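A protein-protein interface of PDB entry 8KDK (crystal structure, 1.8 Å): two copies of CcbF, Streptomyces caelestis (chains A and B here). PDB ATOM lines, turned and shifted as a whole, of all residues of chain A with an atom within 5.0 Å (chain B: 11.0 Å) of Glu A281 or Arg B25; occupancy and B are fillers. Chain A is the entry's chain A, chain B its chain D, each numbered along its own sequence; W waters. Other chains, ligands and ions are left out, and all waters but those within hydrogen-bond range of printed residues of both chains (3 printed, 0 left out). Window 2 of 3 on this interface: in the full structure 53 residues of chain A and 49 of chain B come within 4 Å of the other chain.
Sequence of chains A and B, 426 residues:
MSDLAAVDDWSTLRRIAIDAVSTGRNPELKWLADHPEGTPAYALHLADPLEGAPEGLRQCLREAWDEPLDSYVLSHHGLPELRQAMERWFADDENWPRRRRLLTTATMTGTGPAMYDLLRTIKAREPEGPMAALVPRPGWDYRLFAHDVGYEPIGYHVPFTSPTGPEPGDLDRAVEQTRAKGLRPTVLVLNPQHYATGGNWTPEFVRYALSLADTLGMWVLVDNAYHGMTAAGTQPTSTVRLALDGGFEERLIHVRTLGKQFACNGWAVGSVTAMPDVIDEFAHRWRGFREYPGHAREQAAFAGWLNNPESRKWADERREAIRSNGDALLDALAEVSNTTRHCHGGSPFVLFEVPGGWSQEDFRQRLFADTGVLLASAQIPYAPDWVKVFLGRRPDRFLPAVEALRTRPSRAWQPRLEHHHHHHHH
The side-chain hydroxyl of Ser B22 lies close to the backbone NH of Gly B24. The backbone carbonyl oxygen (O) of Gly B24 lies within hydrogen-bond range of the side-chain amino group (NZ) of Lys B30 (2.7 Å). The backbone carbonyl oxygen (O) of Glu A281 is in hydrogen-bond range of the backbone NH (N) of Trp A286 (3.3 Å).
No position is printed for both chains.
The backbone carbonyl oxygen (O) of Thr B23 sits at hydrogen-bond distance from the backbone NH (N) of His A76, 2.9 Å away. The guanidinium group (NH2) of Arg B25 is in salt-bridge range of the side-chain carboxylate (OD2) of Asp A280 (2.8 Å). OE2 of Glu A281 lies within salt-bridge range of NH2 of Arg B25 (2.7 Å). The side-chain carboxylate (OD1) of Asp B148 is in salt-bridge range of the guanidinium group (NH2) of Arg A285, 2.9 Å away.
Of chain B, only Arg B25 (2.7 Å) comes within 4 Å of Glu A281. Arg B25 touches three residues of chain A. No residue of chain B comes within 4 Å of Thr A121. Val A278 touches none of the printed residues of chain B. Asp A280 touches one residue of chain B. No residue of chain B comes within 4 Å of Ala A283. His A284 touches one residue of chain B. Of the printed residues of chain A, Thr B23 touches His A76 (2.9 Å). Of the printed residues of chain A, Gly B24 touches His A76. Of the printed residues of chain B, Arg A285 touches Asp B148. Of the printed residues of chain B, His A76 touches Ser B22 (3.9 Å), Thr B23 (2.9 Å) and Gly B24 (3.6 Å). Printed residues of chain A within 4 Å of Asp B148: Arg A285. Trp B31 touches none of the printed residues of chain A. Pro B27 touches none of the printed residues of chain A. The nearest residue of chain B that does not touch Glu A281 is Ser B22 (9.3 Å). The nearest residue of chain A that does not touch Arg B25 is His A76 (4.7 Å). The nearest printed residue of chain A that does not touch Gly B24 is Asp A280 (5.4 Å).
Water W1 bridges OD1 of Asp A280 (2.5 Å) and OG of Ser B22 (2.8 Å). Water W2 lies within hydrogen-bond range of ND1 of His A76 (2.8 Å), ND1 of His A284 (2.9 Å) and N of Arg B25 (3.1 Å). Water W3 bridges the backbone carbonyl oxygen (O) of Trp A286 (2.8 Å) and the side-chain carboxylate (OD2) of Asp B148 (3.5 Å).
His A76 touches Ser B22. His A76 touches Gly B24. CD2 of His A284 touches NH1 of Arg B25, at 3.3 Å.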
ATOM      1  N   HIS A  76     -28.430   6.990  18.198  1.00  0.00           N
ATOM      2  CA  HIS A  76     -27.033   7.036  18.641  1.00  0.00           C
ATOM      3  C   HIS A  76     -26.736   8.206  19.593  1.00  0.00           C
ATOM      4  O   HIS A  76     -25.610   8.307  20.099  1.00  0.00           O
ATOM      5  CB  HIS A  76     -26.101   6.997  17.406  1.00  0.00           C
ATOM      6  CG  HIS A  76     -26.077   8.238  16.572  1.00  0.00           C
ATOM      7  ND1 HIS A  76     -25.279   8.351  15.448  1.00  0.00           N
ATOM      8  CD2 HIS A  76     -26.709   9.430  16.703  1.00  0.00           C
ATOM      9  CE1 HIS A  76     -25.435   9.552  14.919  1.00  0.00           C
ATOM     10  NE2 HIS A  76     -26.290  10.229  15.665  1.00  0.00           N
ATOM     11  N   THR A 121     -12.301  12.230  17.936  1.00  0.00           N
ATOM     12  CA  THR A 121     -13.075  12.908  16.895  1.00  0.00           C
ATOM     13  C   THR A 121     -12.307  14.100  16.342  1.00  0.00           C
ATOM     14  O   THR A 121     -12.305  14.343  15.129  1.00  0.00           O
ATOM     15  CB  THR A 121     -14.421  13.373  17.463  1.00  0.00           C
ATOM     16  OG1 THR A 121     -15.143  12.247  17.973  1.00  0.00           O
ATOM     17  CG2 THR A 121     -15.260  14.083  16.395  1.00  0.00           C
ATOM     18  N   ARG A 125     -10.195  15.099  12.497  1.00  0.00           N
ATOM     19  CA  ARG A 125     -10.573  16.277  11.723  1.00  0.00           C
ATOM     20  C   ARG A 125      -9.428  17.261  11.503  1.00  0.00           C
ATOM     21  O   ARG A 125      -9.643  18.328  10.917  1.00  0.00           O
ATOM     22  CB  ARG A 125     -11.715  17.008  12.424  1.00  0.00           C
ATOM     23  CG  ARG A 125     -13.013  16.273  12.416  1.00  0.00           C
ATOM     24  CD  ARG A 125     -13.928  16.912  13.427  1.00  0.00           C
ATOM     25  NE  ARG A 125     -14.609  18.039  12.815  1.00  0.00           N
ATOM     26  CZ  ARG A 125     -15.707  17.927  12.086  1.00  0.00           C
ATOM     27  NH1 ARG A 125     -16.295  16.759  11.903  1.00  0.00           N
ATOM     28  NH2 ARG A 125     -16.229  19.014  11.530  1.00  0.00           N
ATOM     29  N   ASP A 277     -21.961  18.534  13.030  1.00  0.00           N
ATOM     30  CA  ASP A 277     -21.104  17.568  12.354  1.00  0.00           C
ATOM     31  C   ASP A 277     -20.163  16.853  13.322  1.00  0.00           C
ATOM     32  O   ASP A 277     -19.845  15.675  13.124  1.00  0.00           O
ATOM     33  CB  ASP A 277     -20.309  18.285  11.271  1.00  0.00           C
ATOM     34  CG  ASP A 277     -21.119  18.495  10.025  1.00  0.00           C
ATOM     35  OD1 ASP A 277     -22.293  18.064  10.028  1.00  0.00           O
ATOM     36  OD2 ASP A 277     -20.604  19.109   9.062  1.00  0.00           O
ATOM     37  N   VAL A 278     -19.690  17.553  14.354  1.00  0.00           N
ATOM     38  CA  VAL A 278     -18.809  16.946  15.351  1.00  0.00           C
ATOM     39  C   VAL A 278     -19.559  15.897  16.173  1.00  0.00           C
ATOM     40  O   VAL A 278     -19.078  14.778  16.382  1.00  0.00           O
ATOM     41  CB  VAL A 278     -18.206  18.043  16.251  1.00  0.00           C
ATOM     42  CG1 VAL A 278     -17.294  17.434  17.311  1.00  0.00           C
ATOM     43  CG2 VAL A 278     -17.476  19.091  15.413  1.00  0.00           C
ATOM     44  N   ILE A 279     -20.744  16.246  16.676  1.00  0.00           N
ATOM     45  CA  ILE A 279     -21.507  15.272  17.452  1.00  0.00           C
ATOM     46  C   ILE A 279     -21.840  14.051  16.610  1.00  0.00           C
ATOM     47  O   ILE A 279     -21.802  12.912  17.101  1.00  0.00           O
ATOM     48  CB  ILE A 279     -22.774  15.924  18.042  1.00  0.00           C
ATOM     49  CG1 ILE A 279     -22.372  17.025  19.024  1.00  0.00           C
ATOM     50  CG2 ILE A 279     -23.658  14.879  18.697  1.00  0.00           C
ATOM     51  CD1 ILE A 279     -22.106  16.525  20.425  1.00  0.00           C
ATOM     52  N   ASP A 280     -22.187  14.258  15.335  1.00  0.00           N
ATOM     53  CA  ASP A 280     -22.508  13.115  14.482  1.00  0.00           C
ATOM     54  C   ASP A 280     -21.332  12.155  14.357  1.00  0.00           C
ATOM     55  O   ASP A 280     -21.509  10.936  14.448  1.00  0.00           O
ATOM     56  CB  ASP A 280     -22.935  13.580  13.096  1.00  0.00           C
ATOM     57  CG  ASP A 280     -23.617  12.483  12.316  1.00  0.00           C
ATOM     58  OD1 ASP A 280     -24.708  12.047  12.739  1.00  0.00           O
ATOM     59  OD2 ASP A 280     -23.059  12.046  11.293  1.00  0.00           O
ATOM     60  N   GLU A 281     -20.124  12.678  14.119  1.00  0.00           N
ATOM     61  CA  GLU A 281     -18.973  11.779  14.001  1.00  0.00           C
ATOM     62  C   GLU A 281     -18.641  11.128  15.324  1.00  0.00           C
ATOM     63  O   GLU A 281     -18.322   9.936  15.372  1.00  0.00           O
ATOM     64  CB  GLU A 281     -17.741  12.512  13.493  1.00  0.00           C
ATOM     65  CG  GLU A 281     -17.916  13.074  12.127  1.00  0.00           C
ATOM     66  CD  GLU A 281     -17.773  11.994  11.058  1.00  0.00           C
ATOM     67  OE1 GLU A 281     -16.974  11.044  11.264  1.00  0.00           O
ATOM     68  OE2 GLU A 281     -18.449  12.101  10.005  1.00  0.00           O
ATOM     69  N   PHE A 282     -18.670  11.911  16.402  1.00  0.00           N
ATOM     70  CA  PHE A 282     -18.455  11.364  17.740  1.00  0.00           C
ATOM     71  C   PHE A 282     -19.416  10.219  18.005  1.00  0.00           C
ATOM     72  O   PHE A 282     -19.019   9.157  18.496  1.00  0.00           O
ATOM     73  CB  PHE A 282     -18.626  12.501  18.761  1.00  0.00           C
ATOM     74  CG  PHE A 282     -18.910  12.061  20.179  1.00  0.00           C
ATOM     75  CD1 PHE A 282     -17.884  11.659  21.019  1.00  0.00           C
ATOM     76  CD2 PHE A 282     -20.192  12.144  20.701  1.00  0.00           C
ATOM     77  CE1 PHE A 282     -18.145  11.290  22.327  1.00  0.00           C
ATOM     78  CE2 PHE A 282     -20.447  11.766  22.019  1.00  0.00           C
ATOM     79  CZ  PHE A 282     -19.428  11.352  22.824  1.00  0.00           C
ATOM     80  N   ALA A 283     -20.700  10.421  17.680  1.00  0.00           N
ATOM     81  CA  ALA A 283     -21.725   9.446  18.043  1.00  0.00           C
ATOM     82  C   ALA A 283     -21.721   8.244  17.107  1.00  0.00           C
ATOM     83  O   ALA A 283     -21.890   7.103  17.551  1.00  0.00           O
ATOM     84  CB  ALA A 283     -23.113  10.106  18.058  1.00  0.00           C
ATOM     85  N   HIS A 284     -21.521   8.474  15.821  1.00  0.00           N
ATOM     86  CA  HIS A 284     -21.601   7.381  14.866  1.00  0.00           C
ATOM     87  C   HIS A 284     -20.341   6.537  14.869  1.00  0.00           C
ATOM     88  O   HIS A 284     -20.418   5.302  14.867  1.00  0.00           O
ATOM     89  CB  HIS A 284     -21.835   7.902  13.445  1.00  0.00           C
ATOM     90  CG  HIS A 284     -21.707   6.833  12.407  1.00  0.00           C
ATOM     91  ND1 HIS A 284     -22.694   5.897  12.185  1.00  0.00           N
ATOM     92  CD2 HIS A 284     -20.698   6.526  11.555  1.00  0.00           C
ATOM     93  CE1 HIS A 284     -22.302   5.061  11.242  1.00  0.00           C
ATOM     94  NE2 HIS A 284     -21.093   5.419  10.844  1.00  0.00           N
ATOM     95  N   ARG A 285     -19.175   7.192  14.861  1.00  0.00           N
ATOM     96  CA  ARG A 285     -17.911   6.540  14.541  1.00  0.00           C
ATOM     97  C   ARG A 285     -17.037   6.287  15.758  1.00  0.00           C
ATOM     98  O   ARG A 285     -16.521   5.179  15.940  1.00  0.00           O
ATOM     99  CB  ARG A 285     -17.142   7.390  13.511  1.00  0.00           C
ATOM    100  CG  ARG A 285     -15.703   6.935  13.288  1.00  0.00           C
ATOM    101  CD  ARG A 285     -15.689   5.543  12.638  1.00  0.00           C
ATOM    102  NE  ARG A 285     -14.348   5.004  12.431  1.00  0.00           N
ATOM    103  CZ  ARG A 285     -13.633   4.351  13.339  1.00  0.00           C
ATOM    104  NH1 ARG A 285     -14.062   4.192  14.590  1.00  0.00           N
ATOM    105  NH2 ARG A 285     -12.451   3.858  12.990  1.00  0.00           N
ATOM    106  N   TRP A 286     -16.816   7.293  16.595  1.00  0.00           N
ATOM    107  CA  TRP A 286     -15.769   7.126  17.592  1.00  0.00           C
ATOM    108  C   TRP A 286     -16.331   6.436  18.833  1.00  0.00           C
ATOM    109  O   TRP A 286     -15.890   5.340  19.189  1.00  0.00           O
ATOM    110  CB  TRP A 286     -15.106   8.483  17.854  1.00  0.00           C
ATOM    111  CG  TRP A 286     -14.445   8.924  16.556  1.00  0.00           C
ATOM    112  CD1 TRP A 286     -14.790   9.975  15.765  1.00  0.00           C
ATOM    113  CD2 TRP A 286     -13.377   8.242  15.876  1.00  0.00           C
ATOM    114  NE1 TRP A 286     -14.002   9.997  14.624  1.00  0.00           N
ATOM    115  CE2 TRP A 286     -13.118   8.951  14.684  1.00  0.00           C
ATOM    116  CE3 TRP A 286     -12.609   7.110  16.171  1.00  0.00           C
ATOM    117  CZ2 TRP A 286     -12.115   8.570  13.791  1.00  0.00           C
ATOM    118  CZ3 TRP A 286     -11.611   6.721  15.261  1.00  0.00           C
ATOM    119  CH2 TRP A 286     -11.390   7.449  14.086  1.00  0.00           C
ATOM    120  N   ALA B  17     -36.296   5.476  19.501  1.00  0.00           N
ATOM    121  CA  ALA B  17     -35.723   5.719  18.179  1.00  0.00           C
ATOM    122  C   ALA B  17     -36.114   7.028  17.498  1.00  0.00           C
ATOM    123  O   ALA B  17     -35.573   7.321  16.426  1.00  0.00           O
ATOM    124  CB  ALA B  17     -36.075   4.561  17.232  1.00  0.00           C
ATOM    125  N   VAL B  21     -33.639  15.511  16.278  1.00  0.00           N
ATOM    126  CA  VAL B  21     -32.393  15.620  15.540  1.00  0.00           C
ATOM    127  C   VAL B  21     -32.134  14.249  14.935  1.00  0.00           C
ATOM    128  O   VAL B  21     -32.876  13.302  15.218  1.00  0.00           O
ATOM    129  CB  VAL B  21     -31.242  16.048  16.460  1.00  0.00           C
ATOM    130  CG1 VAL B  21     -31.519  17.466  17.001  1.00  0.00           C
ATOM    131  CG2 VAL B  21     -31.037  15.006  17.577  1.00  0.00           C
ATOM    132  N   SER B  22     -31.067  14.122  14.142  1.00  0.00           N
ATOM    133  CA  SER B  22     -30.767  12.848  13.495  1.00  0.00           C
ATOM    134  C   SER B  22     -30.512  11.778  14.540  1.00  0.00           C
ATOM    135  O   SER B  22     -29.770  11.996  15.506  1.00  0.00           O
ATOM    136  CB  SER B  22     -29.555  12.983  12.570  1.00  0.00           C
ATOM    137  OG  SER B  22     -29.163  11.706  12.080  1.00  0.00           O
ATOM    138  N   THR B  23     -31.146  10.624  14.368  1.00  0.00           N
ATOM    139  CA  THR B  23     -30.966   9.553  15.330  1.00  0.00           C
ATOM    140  C   THR B  23     -29.869   8.595  14.910  1.00  0.00           C
ATOM    141  O   THR B  23     -29.568   7.658  15.653  1.00  0.00           O
ATOM    142  CB  THR B  23     -32.273   8.778  15.552  1.00  0.00           C
ATOM    143  OG1 THR B  23     -32.826   8.407  14.288  1.00  0.00           O
ATOM    144  CG2 THR B  23     -33.280   9.649  16.308  1.00  0.00           C
ATOM    145  N   GLY B  24     -29.236   8.836  13.768  1.00  0.00           N
ATOM    146  CA  GLY B  24     -28.214   7.918  13.307  1.00  0.00           C
ATOM    147  C   GLY B  24     -28.196   7.745  11.807  1.00  0.00           C
ATOM    148  O   GLY B  24     -29.092   8.223  11.103  1.00  0.00           O
ATOM    149  N   ARG B  25     -27.185   7.050  11.307  1.00  0.00           N
ATOM    150  CA  ARG B  25     -27.002   6.916   9.868  1.00  0.00           C
ATOM    151  C   ARG B  25     -27.620   5.645   9.314  1.00  0.00           C
ATOM    152  O   ARG B  25     -27.739   5.519   8.089  1.00  0.00           O
ATOM    153  CB  ARG B  25     -25.503   6.961   9.518  1.00  0.00           C
ATOM    154  CG  ARG B  25     -24.776   8.203  10.055  1.00  0.00           C
ATOM    155  CD  ARG B  25     -23.390   8.317   9.458  1.00  0.00           C
ATOM    156  NE  ARG B  25     -22.654   9.464   9.983  1.00  0.00           N
ATOM    157  CZ  ARG B  25     -21.353   9.678   9.817  1.00  0.00           C
ATOM    158  NH1 ARG B  25     -20.590   8.830   9.140  1.00  0.00           N
ATOM    159  NH2 ARG B  25     -20.802  10.768  10.350  1.00  0.00           N
ATOM    160  N   ASN B  26     -28.028   4.721  10.179  1.00  0.00           N
ATOM    161  CA  ASN B  26     -28.616   3.470   9.721  1.00  0.00           C
ATOM    162  C   ASN B  26     -29.927   3.749   8.990  1.00  0.00           C
ATOM    163  O   ASN B  26     -30.717   4.593   9.431  1.00  0.00           O
ATOM    164  CB  ASN B  26     -28.867   2.529  10.903  1.00  0.00           C
ATOM    165  N   PRO B  27     -30.188   3.068   7.874  1.00  0.00           N
ATOM    166  CA  PRO B  27     -31.411   3.353   7.103  1.00  0.00           C
ATOM    167  C   PRO B  27     -32.700   3.073   7.860  1.00  0.00           C
ATOM    168  O   PRO B  27     -33.700   3.772   7.643  1.00  0.00           O
ATOM    169  CB  PRO B  27     -31.275   2.425   5.885  1.00  0.00           C
ATOM    170  CG  PRO B  27     -29.828   2.086   5.820  1.00  0.00           C
ATOM    171  CD  PRO B  27     -29.359   2.034   7.234  1.00  0.00           C
ATOM    172  N   GLU B  28     -32.717   2.050   8.710  1.00  0.00           N
ATOM    173  CA  GLU B  28     -33.940   1.670   9.409  1.00  0.00           C
ATOM    174  C   GLU B  28     -34.465   2.802  10.283  1.00  0.00           C
ATOM    175  O   GLU B  28     -35.674   2.888  10.525  1.00  0.00           O
ATOM    176  CB  GLU B  28     -33.678   0.418  10.254  1.00  0.00           C
ATOM    177  CG  GLU B  28     -33.351  -0.825   9.433  1.00  0.00           C
ATOM    178  CD  GLU B  28     -31.860  -0.952   9.111  1.00  0.00           C
ATOM    179  OE1 GLU B  28     -31.065  -0.099   9.575  1.00  0.00           O
ATOM    180  OE2 GLU B  28     -31.488  -1.897   8.372  1.00  0.00           O
ATOM    181  N   LEU B  29     -33.576   3.669  10.777  1.00  0.00           N
ATOM    182  CA  LEU B  29     -34.010   4.809  11.572  1.00  0.00           C
ATOM    183  C   LEU B  29     -34.818   5.811  10.751  1.00  0.00           C
ATOM    184  O   LEU B  29     -35.705   6.475  11.297  1.00  0.00           O
ATOM    185  CB  LEU B  29     -32.795   5.488  12.196  1.00  0.00           C
ATOM    186  CG  LEU B  29     -32.010   4.666  13.203  1.00  0.00           C
ATOM    187  CD1 LEU B  29     -30.831   5.497  13.602  1.00  0.00           C
ATOM    188  CD2 LEU B  29     -32.861   4.331  14.434  1.00  0.00           C
ATOM    189  N   LYS B  30     -34.520   5.962   9.452  1.00  0.00           N
ATOM    190  CA  LYS B  30     -35.371   6.801   8.612  1.00  0.00           C
ATOM    191  C   LYS B  30     -36.712   6.134   8.356  1.00  0.00           C
ATOM    192  O   LYS B  30     -37.749   6.805   8.324  1.00  0.00           O
ATOM    193  CB  LYS B  30     -34.702   7.118   7.265  1.00  0.00           C
ATOM    194  CG  LYS B  30     -33.182   7.032   7.193  1.00  0.00           C
ATOM    195  CD  LYS B  30     -32.496   8.200   7.883  1.00  0.00           C
ATOM    196  CE  LYS B  30     -30.992   7.972   7.952  1.00  0.00           C
ATOM    197  NZ  LYS B  30     -30.656   7.192   9.179  1.00  0.00           N
ATOM    198  N   TRP B  31     -36.708   4.821   8.115  1.00  0.00           N
ATOM    199  CA  TRP B  31     -37.968   4.107   7.919  1.00  0.00           C
ATOM    200  C   TRP B  31     -38.872   4.260   9.143  1.00  0.00           C
ATOM    201  O   TRP B  31     -40.077   4.500   9.013  1.00  0.00           O
ATOM    202  CB  TRP B  31     -37.689   2.624   7.645  1.00  0.00           C
ATOM    203  CG  TRP B  31     -36.710   2.348   6.497  1.00  0.00           C
ATOM    204  CD1 TRP B  31     -36.240   3.248   5.577  1.00  0.00           C
ATOM    205  CD2 TRP B  31     -36.022   1.115   6.238  1.00  0.00           C
ATOM    206  NE1 TRP B  31     -35.330   2.630   4.727  1.00  0.00           N
ATOM    207  CE2 TRP B  31     -35.179   1.325   5.119  1.00  0.00           C
ATOM    208  CE3 TRP B  31     -36.048  -0.154   6.829  1.00  0.00           C
ATOM    209  CZ2 TRP B  31     -34.379   0.314   4.587  1.00  0.00           C
ATOM    210  CZ3 TRP B  31     -35.246  -1.162   6.293  1.00  0.00           C
ATOM    211  CH2 TRP B  31     -34.427  -0.918   5.188  1.00  0.00           C
ATOM    212  N   LEU B  32     -38.300   4.129  10.344  1.00  0.00           N
ATOM    213  CA  LEU B  32     -39.077   4.301  11.573  1.00  0.00           C
ATOM    214  C   LEU B  32     -39.616   5.721  11.694  1.00  0.00           C
ATOM    215  O   LEU B  32     -40.761   5.924  12.108  1.00  0.00           O
ATOM    216  CB  LEU B  32     -38.206   3.948  12.792  1.00  0.00           C
ATOM    217  CG  LEU B  32     -37.821   2.465  12.938  1.00  0.00           C
ATOM    218  CD1 LEU B  32     -36.685   2.283  13.891  1.00  0.00           C
ATOM    219  CD2 LEU B  32     -39.000   1.620  13.419  1.00  0.00           C
ATOM    220  N   ASP B 148      -9.322  -0.293  15.653  1.00  0.00           N
ATOM    221  CA  ASP B 148      -9.101   0.937  16.408  1.00  0.00           C
ATOM    222  C   ASP B 148      -8.026   0.796  17.475  1.00  0.00           C
ATOM    223  O   ASP B 148      -7.514   1.817  17.943  1.00  0.00           O
ATOM    224  CB  ASP B 148     -10.400   1.415  17.068  1.00  0.00           C
ATOM    225  CG  ASP B 148     -11.307   2.143  16.092  1.00  0.00           C
ATOM    226  OD1 ASP B 148     -10.784   2.738  15.121  1.00  0.00           O
ATOM    227  OD2 ASP B 148     -12.534   2.129  16.300  1.00  0.00           O
ATOM    228  N   GLU B 361     -31.890  -4.216   1.026  1.00  0.00           N
ATOM    229  CA  GLU B 361     -32.375  -2.991   1.660  1.00  0.00           C
ATOM    230  C   GLU B 361     -33.730  -2.565   1.099  1.00  0.00           C
ATOM    231  O   GLU B 361     -34.669  -2.291   1.864  1.00  0.00           O
ATOM    232  CB  GLU B 361     -31.355  -1.859   1.516  1.00  0.00           C
ATOM    233  CG  GLU B 361     -31.657  -0.721   2.472  1.00  0.00           C
ATOM    234  CD  GLU B 361     -30.546   0.308   2.594  1.00  0.00           C
ATOM    235  OE1 GLU B 361     -29.373  -0.063   2.838  1.00  0.00           O
ATOM    236  OE2 GLU B 361     -30.864   1.504   2.485  1.00  0.00           O
ATOM    237  N   ARG B 364     -36.364  -4.960   2.475  1.00  0.00           N
ATOM    238  CA  ARG B 364     -36.805  -4.758   3.853  1.00  0.00           C
ATOM    239  C   ARG B 364     -37.602  -3.470   3.992  1.00  0.00           C
ATOM    240  O   ARG B 364     -38.597  -3.426   4.725  1.00  0.00           O
ATOM    241  CB  ARG B 364     -35.610  -4.770   4.800  1.00  0.00           C
ATOM    242  CG  ARG B 364     -34.937  -6.131   4.832  1.00  0.00           C
ATOM    243  CD  ARG B 364     -33.789  -6.160   5.807  1.00  0.00           C
ATOM    244  NE  ARG B 364     -32.735  -5.219   5.441  1.00  0.00           N
ATOM    245  CZ  ARG B 364     -32.399  -4.166   6.177  1.00  0.00           C
ATOM    246  NH1 ARG B 364     -33.030  -3.877   7.311  1.00  0.00           N
ATOM    247  NH2 ARG B 364     -31.421  -3.371   5.755  1.00  0.00           N
HETATM  248  O   HOH W   1     -26.529  10.829  11.450  1.00  0.00           O
HETATM  249  O   HOH W   2     -25.184   6.307  13.592  1.00  0.00           O
HETATM  250  O   HOH W   3     -14.077   3.200  19.218  1.00  0.00           O
